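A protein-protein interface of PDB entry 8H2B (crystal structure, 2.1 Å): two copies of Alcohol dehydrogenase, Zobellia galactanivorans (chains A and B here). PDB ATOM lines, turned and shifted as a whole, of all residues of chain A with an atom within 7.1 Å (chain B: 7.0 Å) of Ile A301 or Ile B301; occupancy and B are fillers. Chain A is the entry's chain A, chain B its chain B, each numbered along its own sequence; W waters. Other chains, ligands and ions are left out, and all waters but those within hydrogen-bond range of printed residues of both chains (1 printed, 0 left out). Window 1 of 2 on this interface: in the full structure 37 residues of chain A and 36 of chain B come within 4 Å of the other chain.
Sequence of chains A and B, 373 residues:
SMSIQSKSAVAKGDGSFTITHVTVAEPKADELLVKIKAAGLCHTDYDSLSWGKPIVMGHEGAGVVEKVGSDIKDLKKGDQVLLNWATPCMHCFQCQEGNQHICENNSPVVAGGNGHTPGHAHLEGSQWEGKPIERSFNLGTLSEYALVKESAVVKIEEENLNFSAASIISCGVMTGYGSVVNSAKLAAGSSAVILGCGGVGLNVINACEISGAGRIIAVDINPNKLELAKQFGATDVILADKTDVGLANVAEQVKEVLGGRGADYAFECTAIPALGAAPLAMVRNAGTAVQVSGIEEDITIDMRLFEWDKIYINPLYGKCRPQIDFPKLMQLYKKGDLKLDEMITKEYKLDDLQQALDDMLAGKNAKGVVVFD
O of Glu A297 sits at hydrogen-bond distance from N of Met B303 (3.0 Å). The backbone NH (N) of Asp B302 sits close to the side-chain carboxylate (OD1) of Asp A298 (3.4 Å). The backbone carbonyl oxygen of Ile A299 sits at hydrogen-bond distance from the backbone NH of Ile B301, 2.9 Å away. The backbone carbonyl oxygen (O) of Ile B299 sits at hydrogen-bond distance from the backbone NH (N) of Ile A301 (2.9 Å). OD1 of Asp B298 lies close to N of Asp A302, at 3.2 Å. The backbone NH of Met A303 lies within hydrogen-bond range of the backbone carbonyl oxygen of Glu B297, 2.9 Å away. O of Ile B295 sits at hydrogen-bond distance from N of Arg A304, at 3.4 Å. N of Tyr B312 is in hydrogen-bond range of O of Tyr A312, 2.9 Å away. The backbone carbonyl oxygen (O) of Met A303 lies close to the backbone carbonyl oxygen (O) of Ile B295, at 3.4 Å.
Ala A277 touches none of the printed residues of chain B. Of the printed residues of chain B, Ile A299 touches Ile B299, Thr B300, Ile B301 and Met B303. Of the printed residues of chain B, Ile A301 touches Glu B297, Asp B298, Ile B299, Ile B301 and Met B303. Of the printed residues of chain B, Arg A304 touches Ile B295. Printed residues of chain A within 4 Å of Ile B299: Ile A299, Thr A300, Ile A301 and Met A303. Of the printed residues of chain A, Ile B301 touches Glu A297 (3.6 Å), Asp A298 (3.3 Å), Ile A299 (2.9 Å), Ile A301 (3.6 Å) and Met A303 (3.9 Å). The nearest printed residue of chain B that does not touch Ile A301 is Thr B300 (5.0 Å).
Glu A297 touches Ile B301, and with the chains exchanged Ile A301 touches Glu B297. Glu A297 touches Met B303, and with the chains exchanged Met A303 touches Glu B297. Asp A298 touches Asp B302, and with the chains exchanged Asp A302 touches Asp B298. Met A303 touches Tyr B312, and with the chains exchanged Tyr A312 touches Met B303. Positions printed for both chains: 276, 277, 280, 297, 298, 299, 300, 301, 302, 303, 304, 305, 306 and 312.
The backbone carbonyl oxygen of Gly A276 is in hydrogen-bond range of the side-chain hydroxyl of Tyr A312 (2.8 Å). The backbone NH of Arg A304 is in hydrogen-bond range of the side-chain carboxylate of Asp A302 (3.0 Å). The backbone carbonyl oxygen (O) of Gly B276 is in hydrogen-bond range of the side-chain hydroxyl (OH) of Tyr B312, 2.6 Å away. The side-chain carboxylate (OD2) of Asp B302 is in salt-bridge range of the guanidinium group (NH2) of Arg B304 (2.9 Å).
Of the 15 printed residues of chain B, 10 touch a printed residue of chain A. Printed residues of chain B that touch a printed residue of chain A: Ile B295, Glu B297, Asp B298, Ile B299, Thr B300, Ile B301, Asp B302, Met B303, Phe B306 and Tyr B312. Among the printed residues, no Asp or Glu carboxylate lies within 4 Å of a Lys or Arg side-chain nitrogen of the other chain.
Water W1 bridges O of Met A303 and N of Ile B295.
Asp A298 touches Thr B300 (CB to CG2, 3.7 Å). CA of Asp A298 touches O of Ile B301, at 3.3 Å. O of Ile A299 touches CA of Thr B300 (3.5 Å). CB of Asp B298 touches CG2 of Thr A300 (3.8 Å). Ile A301 touches Glu B297 (O to O, 3.7 Å). Ile B299 touches Met A303 (CG1 to SD, 3.7 Å). Met A303 touches Ile B301. OH of Tyr B312 touches CE of Met A303, at 3.5 Å. Phe A306 touches Tyr B312 (CE1 to CD1, 3.4 Å). Tyr A312 touches Met B303 (OH to CE, 3.7 Å).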
ATOM      1  N   ALA A 274      -4.281   1.147  -5.175  1.00  0.00           N
ATOM      2  CA  ALA A 274      -5.133   2.250  -4.743  1.00  0.00           C
ATOM      3  C   ALA A 274      -6.552   1.806  -4.430  1.00  0.00           C
ATOM      4  O   ALA A 274      -7.290   2.558  -3.784  1.00  0.00           O
ATOM      5  CB  ALA A 274      -5.178   3.346  -5.805  1.00  0.00           C
ATOM      6  N   GLY A 276      -7.499  -0.743  -2.549  1.00  0.00           N
ATOM      7  CA  GLY A 276      -7.494  -1.692  -1.451  1.00  0.00           C
ATOM      8  C   GLY A 276      -8.657  -1.541  -0.497  1.00  0.00           C
ATOM      9  O   GLY A 276      -9.104  -2.527   0.100  1.00  0.00           O
ATOM     10  N   ALA A 277      -9.162  -0.321  -0.337  1.00  0.00           N
ATOM     11  CA  ALA A 277     -10.294  -0.058   0.544  1.00  0.00           C
ATOM     12  C   ALA A 277     -11.642  -0.065  -0.178  1.00  0.00           C
ATOM     13  O   ALA A 277     -12.687  -0.042   0.487  1.00  0.00           O
ATOM     14  CB  ALA A 277     -10.092   1.280   1.254  1.00  0.00           C
ATOM     15  N   ALA A 278     -11.645  -0.153  -1.509  1.00  0.00           N
ATOM     16  CA  ALA A 278     -12.893  -0.140  -2.266  1.00  0.00           C
ATOM     17  C   ALA A 278     -13.949  -1.143  -1.795  1.00  0.00           C
ATOM     18  O   ALA A 278     -15.141  -0.792  -1.833  1.00  0.00           O
ATOM     19  CB  ALA A 278     -12.600  -0.363  -3.756  1.00  0.00           C
ATOM     20  N   LEU A 280     -14.855  -1.890   1.083  1.00  0.00           N
ATOM     21  CA  LEU A 280     -15.572  -1.328   2.224  1.00  0.00           C
ATOM     22  C   LEU A 280     -16.661  -0.370   1.762  1.00  0.00           C
ATOM     23  O   LEU A 280     -17.734  -0.284   2.385  1.00  0.00           O
ATOM     24  CB  LEU A 280     -14.598  -0.613   3.161  1.00  0.00           C
ATOM     25  CG  LEU A 280     -13.592  -1.449   3.957  1.00  0.00           C
ATOM     26  CD1 LEU A 280     -12.551  -0.502   4.489  1.00  0.00           C
ATOM     27  CD2 LEU A 280     -14.247  -2.179   5.122  1.00  0.00           C
ATOM     28  N   GLU A 297       2.102  -1.554  -0.214  1.00  0.00           N
ATOM     29  CA  GLU A 297       2.445  -0.148  -0.365  1.00  0.00           C
ATOM     30  C   GLU A 297       1.700   0.662   0.676  1.00  0.00           C
ATOM     31  O   GLU A 297       0.739   0.185   1.281  1.00  0.00           O
ATOM     32  CB  GLU A 297       2.082   0.384  -1.752  1.00  0.00           C
ATOM     33  CG  GLU A 297       2.757  -0.364  -2.863  1.00  0.00           C
ATOM     34  CD  GLU A 297       2.111  -0.104  -4.189  1.00  0.00           C
ATOM     35  OE1 GLU A 297       1.192   0.746  -4.236  1.00  0.00           O
ATOM     36  OE2 GLU A 297       2.512  -0.761  -5.174  1.00  0.00           O
ATOM     37  N   ASP A 298       2.156   1.896   0.875  1.00  0.00           N
ATOM     38  CA  ASP A 298       1.372   2.873   1.620  1.00  0.00           C
ATOM     39  C   ASP A 298       0.262   3.395   0.721  1.00  0.00           C
ATOM     40  O   ASP A 298       0.514   3.785  -0.423  1.00  0.00           O
ATOM     41  CB  ASP A 298       2.236   4.052   2.085  1.00  0.00           C
ATOM     42  CG  ASP A 298       3.248   3.673   3.156  1.00  0.00           C
ATOM     43  OD1 ASP A 298       2.873   3.009   4.151  1.00  0.00           O
ATOM     44  OD2 ASP A 298       4.415   4.106   3.032  1.00  0.00           O
ATOM     45  N   ILE A 299      -0.968   3.375   1.217  1.00  0.00           N
ATOM     46  CA  ILE A 299      -2.092   3.971   0.512  1.00  0.00           C
ATOM     47  C   ILE A 299      -2.870   4.822   1.507  1.00  0.00           C
ATOM     48  O   ILE A 299      -2.859   4.570   2.718  1.00  0.00           O
ATOM     49  CB  ILE A 299      -3.014   2.925  -0.176  1.00  0.00           C
ATOM     50  CG1 ILE A 299      -3.932   2.238   0.832  1.00  0.00           C
ATOM     51  CG2 ILE A 299      -2.205   1.892  -0.974  1.00  0.00           C
ATOM     52  CD1 ILE A 299      -4.861   1.207   0.209  1.00  0.00           C
ATOM     53  N   THR A 300      -3.502   5.871   0.995  1.00  0.00           N
ATOM     54  CA  THR A 300      -4.337   6.750   1.804  1.00  0.00           C
ATOM     55  C   THR A 300      -5.764   6.217   1.807  1.00  0.00           C
ATOM     56  O   THR A 300      -6.298   5.857   0.755  1.00  0.00           O
ATOM     57  CB  THR A 300      -4.310   8.171   1.249  1.00  0.00           C
ATOM     58  OG1 THR A 300      -2.957   8.616   1.188  1.00  0.00           O
ATOM     59  CG2 THR A 300      -5.127   9.130   2.127  1.00  0.00           C
ATOM     60  N   ILE A 301      -6.371   6.141   2.986  1.00  0.00           N
ATOM     61  CA  ILE A 301      -7.702   5.566   3.143  1.00  0.00           C
ATOM     62  C   ILE A 301      -8.570   6.518   3.950  1.00  0.00           C
ATOM     63  O   ILE A 301      -8.163   6.980   5.024  1.00  0.00           O
ATOM     64  CB  ILE A 301      -7.647   4.190   3.832  1.00  0.00           C
ATOM     65  CG1 ILE A 301      -6.600   3.302   3.177  1.00  0.00           C
ATOM     66  CG2 ILE A 301      -9.012   3.536   3.837  1.00  0.00           C
ATOM     67  CD1 ILE A 301      -6.609   1.883   3.703  1.00  0.00           C
ATOM     68  N   ASP A 302      -9.764   6.802   3.438  1.00  0.00           N
ATOM     69  CA  ASP A 302     -10.784   7.486   4.221  1.00  0.00           C
ATOM     70  C   ASP A 302     -11.281   6.523   5.291  1.00  0.00           C
ATOM     71  O   ASP A 302     -11.966   5.545   4.984  1.00  0.00           O
ATOM     72  CB  ASP A 302     -11.914   7.961   3.304  1.00  0.00           C
ATOM     73  CG  ASP A 302     -13.113   8.533   4.068  1.00  0.00           C
ATOM     74  OD1 ASP A 302     -13.030   8.741   5.297  1.00  0.00           O
ATOM     75  OD2 ASP A 302     -14.144   8.815   3.426  1.00  0.00           O
ATOM     76  N   MET A 303     -10.943   6.789   6.553  1.00  0.00           N
ATOM     77  CA  MET A 303     -11.243   5.819   7.603  1.00  0.00           C
ATOM     78  C   MET A 303     -12.735   5.713   7.879  1.00  0.00           C
ATOM     79  O   MET A 303     -13.171   4.753   8.536  1.00  0.00           O
ATOM     80  CB  MET A 303     -10.486   6.195   8.877  1.00  0.00           C
ATOM     81  CG  MET A 303      -8.996   5.923   8.841  1.00  0.00           C
ATOM     82  SD  MET A 303      -8.466   4.296   8.238  1.00  0.00           S
ATOM     83  CE  MET A 303      -8.779   3.334   9.720  1.00  0.00           C
ATOM     84  N   ARG A 304     -13.520   6.690   7.408  1.00  0.00           N
ATOM     85  CA  ARG A 304     -14.972   6.590   7.453  1.00  0.00           C
ATOM     86  C   ARG A 304     -15.461   5.305   6.797  1.00  0.00           C
ATOM     87  O   ARG A 304     -16.535   4.798   7.149  1.00  0.00           O
ATOM     88  CB  ARG A 304     -15.605   7.787   6.736  1.00  0.00           C
ATOM     89  CG  ARG A 304     -15.728   9.078   7.534  1.00  0.00           C
ATOM     90  CD  ARG A 304     -16.482  10.162   6.724  1.00  0.00           C
ATOM     91  NE  ARG A 304     -17.939  10.024   6.816  1.00  0.00           N
ATOM     92  CZ  ARG A 304     -18.789  10.201   5.803  1.00  0.00           C
ATOM     93  NH1 ARG A 304     -18.341  10.535   4.598  1.00  0.00           N
ATOM     94  NH2 ARG A 304     -20.094  10.051   5.994  1.00  0.00           N
ATOM     95  N   LEU A 305     -14.721   4.794   5.806  1.00  0.00           N
ATOM     96  CA  LEU A 305     -15.133   3.568   5.127  1.00  0.00           C
ATOM     97  C   LEU A 305     -15.241   2.390   6.084  1.00  0.00           C
ATOM     98  O   LEU A 305     -16.022   1.468   5.835  1.00  0.00           O
ATOM     99  CB  LEU A 305     -14.162   3.227   3.996  1.00  0.00           C
ATOM    100  CG  LEU A 305     -14.111   4.244   2.846  1.00  0.00           C
ATOM    101  CD1 LEU A 305     -12.959   3.949   1.913  1.00  0.00           C
ATOM    102  CD2 LEU A 305     -15.426   4.302   2.090  1.00  0.00           C
ATOM    103  N   PHE A 306     -14.461   2.386   7.170  1.00  0.00           N
ATOM    104  CA  PHE A 306     -14.587   1.326   8.165  1.00  0.00           C
ATOM    105  C   PHE A 306     -15.817   1.485   9.048  1.00  0.00           C
ATOM    106  O   PHE A 306     -16.247   0.510   9.676  1.00  0.00           O
ATOM    107  CB  PHE A 306     -13.331   1.284   9.024  1.00  0.00           C
ATOM    108  CG  PHE A 306     -12.155   0.744   8.299  1.00  0.00           C
ATOM    109  CD1 PHE A 306     -12.054  -0.624   8.045  1.00  0.00           C
ATOM    110  CD2 PHE A 306     -11.166   1.597   7.831  1.00  0.00           C
ATOM    111  CE1 PHE A 306     -10.954  -1.139   7.366  1.00  0.00           C
ATOM    112  CE2 PHE A 306     -10.057   1.096   7.162  1.00  0.00           C
ATOM    113  CZ  PHE A 306      -9.952  -0.269   6.914  1.00  0.00           C
ATOM    114  N   TYR A 312     -13.149  -6.529   7.775  1.00  0.00           N
ATOM    115  CA  TYR A 312     -12.196  -6.421   6.686  1.00  0.00           C
ATOM    116  C   TYR A 312     -11.087  -7.449   6.874  1.00  0.00           C
ATOM    117  O   TYR A 312     -10.520  -7.562   7.962  1.00  0.00           O
ATOM    118  CB  TYR A 312     -11.640  -5.012   6.640  1.00  0.00           C
ATOM    119  CG  TYR A 312     -10.745  -4.716   5.475  1.00  0.00           C
ATOM    120  CD1 TYR A 312     -11.251  -4.197   4.293  1.00  0.00           C
ATOM    121  CD2 TYR A 312      -9.386  -4.922   5.575  1.00  0.00           C
ATOM    122  CE1 TYR A 312     -10.414  -3.884   3.242  1.00  0.00           C
ATOM    123  CE2 TYR A 312      -8.544  -4.638   4.542  1.00  0.00           C
ATOM    124  CZ  TYR A 312      -9.056  -4.122   3.377  1.00  0.00           C
ATOM    125  OH  TYR A 312      -8.182  -3.819   2.363  1.00  0.00           O
ATOM    126  N   GLY B 276      -4.929   4.487  13.756  1.00  0.00           N
ATOM    127  CA  GLY B 276      -6.055   3.620  13.456  1.00  0.00           C
ATOM    128  C   GLY B 276      -5.664   2.233  12.994  1.00  0.00           C
ATOM    129  O   GLY B 276      -6.399   1.265  13.230  1.00  0.00           O
ATOM    130  N   ALA B 277      -4.512   2.113  12.337  1.00  0.00           N
ATOM    131  CA  ALA B 277      -4.000   0.831  11.869  1.00  0.00           C
ATOM    132  C   ALA B 277      -3.113   0.127  12.890  1.00  0.00           C
ATOM    133  O   ALA B 277      -2.743  -1.030  12.669  1.00  0.00           O
ATOM    134  CB  ALA B 277      -3.213   1.029  10.566  1.00  0.00           C
ATOM    135  N   LEU B 280      -3.221  -3.679  14.037  1.00  0.00           N
ATOM    136  CA  LEU B 280      -2.766  -4.696  13.086  1.00  0.00           C
ATOM    137  C   LEU B 280      -1.301  -5.059  13.310  1.00  0.00           C
ATOM    138  O   LEU B 280      -0.915  -6.228  13.152  1.00  0.00           O
ATOM    139  CB  LEU B 280      -2.964  -4.194  11.655  1.00  0.00           C
ATOM    140  CG  LEU B 280      -4.424  -4.068  11.183  1.00  0.00           C
ATOM    141  CD1 LEU B 280      -4.496  -3.264   9.908  1.00  0.00           C
ATOM    142  CD2 LEU B 280      -5.030  -5.448  10.958  1.00  0.00           C
ATOM    143  N   ILE B 295     -12.559   6.744  13.374  1.00  0.00           N
ATOM    144  CA  ILE B 295     -11.758   7.778  12.730  1.00  0.00           C
ATOM    145  C   ILE B 295     -12.480   8.243  11.473  1.00  0.00           C
ATOM    146  O   ILE B 295     -12.856   7.419  10.632  1.00  0.00           O
ATOM    147  CB  ILE B 295     -10.353   7.253  12.401  1.00  0.00           C
ATOM    148  CG1 ILE B 295      -9.686   6.782  13.691  1.00  0.00           C
ATOM    149  CG2 ILE B 295      -9.517   8.313  11.691  1.00  0.00           C
ATOM    150  CD1 ILE B 295      -8.556   5.885  13.473  1.00  0.00           C
ATOM    151  N   GLU B 297     -11.086  10.618   9.377  1.00  0.00           N
ATOM    152  CA  GLU B 297     -10.079  11.300   8.584  1.00  0.00           C
ATOM    153  C   GLU B 297      -9.522  10.359   7.526  1.00  0.00           C
ATOM    154  O   GLU B 297      -9.679   9.140   7.605  1.00  0.00           O
ATOM    155  CB  GLU B 297      -8.938  11.779   9.482  1.00  0.00           C
ATOM    156  CG  GLU B 297      -9.289  12.949  10.365  1.00  0.00           C
ATOM    157  CD  GLU B 297      -8.104  13.392  11.182  1.00  0.00           C
ATOM    158  OE1 GLU B 297      -6.968  13.052  10.788  1.00  0.00           O
ATOM    159  OE2 GLU B 297      -8.306  14.068  12.215  1.00  0.00           O
ATOM    160  N   ASP B 298      -8.845  10.944   6.542  1.00  0.00           N
ATOM    161  CA  ASP B 298      -7.900  10.200   5.719  1.00  0.00           C
ATOM    162  C   ASP B 298      -6.630   9.946   6.510  1.00  0.00           C
ATOM    163  O   ASP B 298      -6.120  10.842   7.193  1.00  0.00           O
ATOM    164  CB  ASP B 298      -7.542  10.970   4.446  1.00  0.00           C
ATOM    165  CG  ASP B 298      -8.687  11.026   3.445  1.00  0.00           C
ATOM    166  OD1 ASP B 298      -9.368  10.004   3.246  1.00  0.00           O
ATOM    167  OD2 ASP B 298      -8.900  12.094   2.841  1.00  0.00           O
ATOM    168  N   ILE B 299      -6.101   8.726   6.412  1.00  0.00           N
ATOM    169  CA  ILE B 299      -4.788   8.423   6.974  1.00  0.00           C
ATOM    170  C   ILE B 299      -4.048   7.520   6.002  1.00  0.00           C
ATOM    171  O   ILE B 299      -4.645   6.844   5.163  1.00  0.00           O
ATOM    172  CB  ILE B 299      -4.849   7.752   8.369  1.00  0.00           C
ATOM    173  CG1 ILE B 299      -5.335   6.303   8.252  1.00  0.00           C
ATOM    174  CG2 ILE B 299      -5.696   8.562   9.356  1.00  0.00           C
ATOM    175  CD1 ILE B 299      -5.083   5.461   9.500  1.00  0.00           C
ATOM    176  N   THR B 300      -2.727   7.511   6.129  1.00  0.00           N
ATOM    177  CA  THR B 300      -1.894   6.666   5.294  1.00  0.00           C
ATOM    178  C   THR B 300      -1.630   5.364   6.037  1.00  0.00           C
ATOM    179  O   THR B 300      -1.262   5.379   7.213  1.00  0.00           O
ATOM    180  CB  THR B 300      -0.581   7.375   4.954  1.00  0.00           C
ATOM    181  OG1 THR B 300      -0.877   8.563   4.209  1.00  0.00           O
ATOM    182  CG2 THR B 300       0.315   6.472   4.118  1.00  0.00           C
ATOM    183  N   ILE B 301      -1.835   4.241   5.361  1.00  0.00           N
ATOM    184  CA  ILE B 301      -1.667   2.928   5.971  1.00  0.00           C
ATOM    185  C   ILE B 301      -0.675   2.131   5.143  1.00  0.00           C
ATOM    186  O   ILE B 301      -0.803   2.064   3.913  1.00  0.00           O
ATOM    187  CB  ILE B 301      -3.002   2.174   6.075  1.00  0.00           C
ATOM    188  CG1 ILE B 301      -3.991   2.978   6.918  1.00  0.00           C
ATOM    189  CG2 ILE B 301      -2.785   0.754   6.633  1.00  0.00           C
ATOM    190  CD1 ILE B 301      -5.348   2.314   7.063  1.00  0.00           C
ATOM    191  N   ASP B 302       0.304   1.523   5.816  1.00  0.00           N
ATOM    192  CA  ASP B 302       1.123   0.494   5.181  1.00  0.00           C
ATOM    193  C   ASP B 302       0.277  -0.767   5.043  1.00  0.00           C
ATOM    194  O   ASP B 302       0.008  -1.459   6.031  1.00  0.00           O
ATOM    195  CB  ASP B 302       2.383   0.246   6.008  1.00  0.00           C
ATOM    196  CG  ASP B 302       3.246  -0.893   5.465  1.00  0.00           C
ATOM    197  OD1 ASP B 302       2.981  -1.420   4.361  1.00  0.00           O
ATOM    198  OD2 ASP B 302       4.228  -1.246   6.138  1.00  0.00           O
ATOM    199  N   MET B 303      -0.156  -1.072   3.818  1.00  0.00           N
ATOM    200  CA  MET B 303      -1.119  -2.150   3.621  1.00  0.00           C
ATOM    201  C   MET B 303      -0.531  -3.522   3.902  1.00  0.00           C
ATOM    202  O   MET B 303      -1.294  -4.488   3.995  1.00  0.00           O
ATOM    203  CB  MET B 303      -1.670  -2.098   2.200  1.00  0.00           C
ATOM    204  CG  MET B 303      -2.452  -0.833   1.969  1.00  0.00           C
ATOM    205  SD  MET B 303      -3.928  -0.721   3.003  1.00  0.00           S
ATOM    206  CE  MET B 303      -4.934  -2.018   2.276  1.00  0.00           C
ATOM    207  N   ARG B 304       0.795  -3.631   4.034  1.00  0.00           N
ATOM    208  CA  ARG B 304       1.403  -4.869   4.511  1.00  0.00           C
ATOM    209  C   ARG B 304       0.902  -5.256   5.893  1.00  0.00           C
ATOM    210  O   ARG B 304       0.954  -6.442   6.256  1.00  0.00           O
ATOM    211  CB  ARG B 304       2.927  -4.741   4.551  1.00  0.00           C
ATOM    212  CG  ARG B 304       3.650  -5.175   3.284  1.00  0.00           C
ATOM    213  CD  ARG B 304       5.161  -4.958   3.407  1.00  0.00           C
ATOM    214  NE  ARG B 304       5.448  -3.668   4.027  1.00  0.00           N
ATOM    215  CZ  ARG B 304       6.646  -3.276   4.446  1.00  0.00           C
ATOM    216  NH1 ARG B 304       7.703  -4.074   4.312  1.00  0.00           N
ATOM    217  NH2 ARG B 304       6.783  -2.077   4.998  1.00  0.00           N
ATOM    218  N   LEU B 305       0.440  -4.278   6.676  1.00  0.00           N
ATOM    219  CA  LEU B 305      -0.080  -4.565   8.008  1.00  0.00           C
ATOM    220  C   LEU B 305      -1.288  -5.489   7.981  1.00  0.00           C
ATOM    221  O   LEU B 305      -1.536  -6.180   8.975  1.00  0.00           O
ATOM    222  CB  LEU B 305      -0.453  -3.265   8.714  1.00  0.00           C
ATOM    223  CG  LEU B 305       0.711  -2.386   9.153  1.00  0.00           C
ATOM    224  CD1 LEU B 305       0.180  -1.035   9.576  1.00  0.00           C
ATOM    225  CD2 LEU B 305       1.491  -3.058  10.289  1.00  0.00           C
ATOM    226  N   PHE B 306      -2.042  -5.520   6.875  1.00  0.00           N
ATOM    227  CA  PHE B 306      -3.194  -6.415   6.771  1.00  0.00           C
ATOM    228  C   PHE B 306      -2.812  -7.841   6.393  1.00  0.00           C
ATOM    229  O   PHE B 306      -3.608  -8.760   6.614  1.00  0.00           O
ATOM    230  CB  PHE B 306      -4.176  -5.892   5.731  1.00  0.00           C
ATOM    231  CG  PHE B 306      -4.910  -4.673   6.157  1.00  0.00           C
ATOM    232  CD1 PHE B 306      -6.019  -4.773   6.991  1.00  0.00           C
ATOM    233  CD2 PHE B 306      -4.482  -3.412   5.740  1.00  0.00           C
ATOM    234  CE1 PHE B 306      -6.716  -3.634   7.368  1.00  0.00           C
ATOM    235  CE2 PHE B 306      -5.166  -2.271   6.119  1.00  0.00           C
ATOM    236  CZ  PHE B 306      -6.284  -2.382   6.937  1.00  0.00           C
ATOM    237  N   TYR B 312      -9.948  -7.122  10.762  1.00  0.00           N
ATOM    238  CA  TYR B 312      -9.965  -5.753  11.254  1.00  0.00           C
ATOM    239  C   TYR B 312     -11.408  -5.268  11.291  1.00  0.00           C
ATOM    240  O   TYR B 312     -12.155  -5.449  10.315  1.00  0.00           O
ATOM    241  CB  TYR B 312      -9.106  -4.863  10.356  1.00  0.00           C
ATOM    242  CG  TYR B 312      -8.951  -3.411  10.779  1.00  0.00           C
ATOM    243  CD1 TYR B 312      -9.851  -2.448  10.346  1.00  0.00           C
ATOM    244  CD2 TYR B 312      -7.893  -3.005  11.587  1.00  0.00           C
ATOM    245  CE1 TYR B 312      -9.710  -1.124  10.711  1.00  0.00           C
ATOM    246  CE2 TYR B 312      -7.735  -1.688  11.951  1.00  0.00           C
ATOM    247  CZ  TYR B 312      -8.660  -0.751  11.510  1.00  0.00           C
ATOM    248  OH  TYR B 312      -8.523   0.568  11.843  1.00  0.00           O
HETATM  249  O   HOH W   1     -12.760   4.445  11.390  1.00  0.00           O
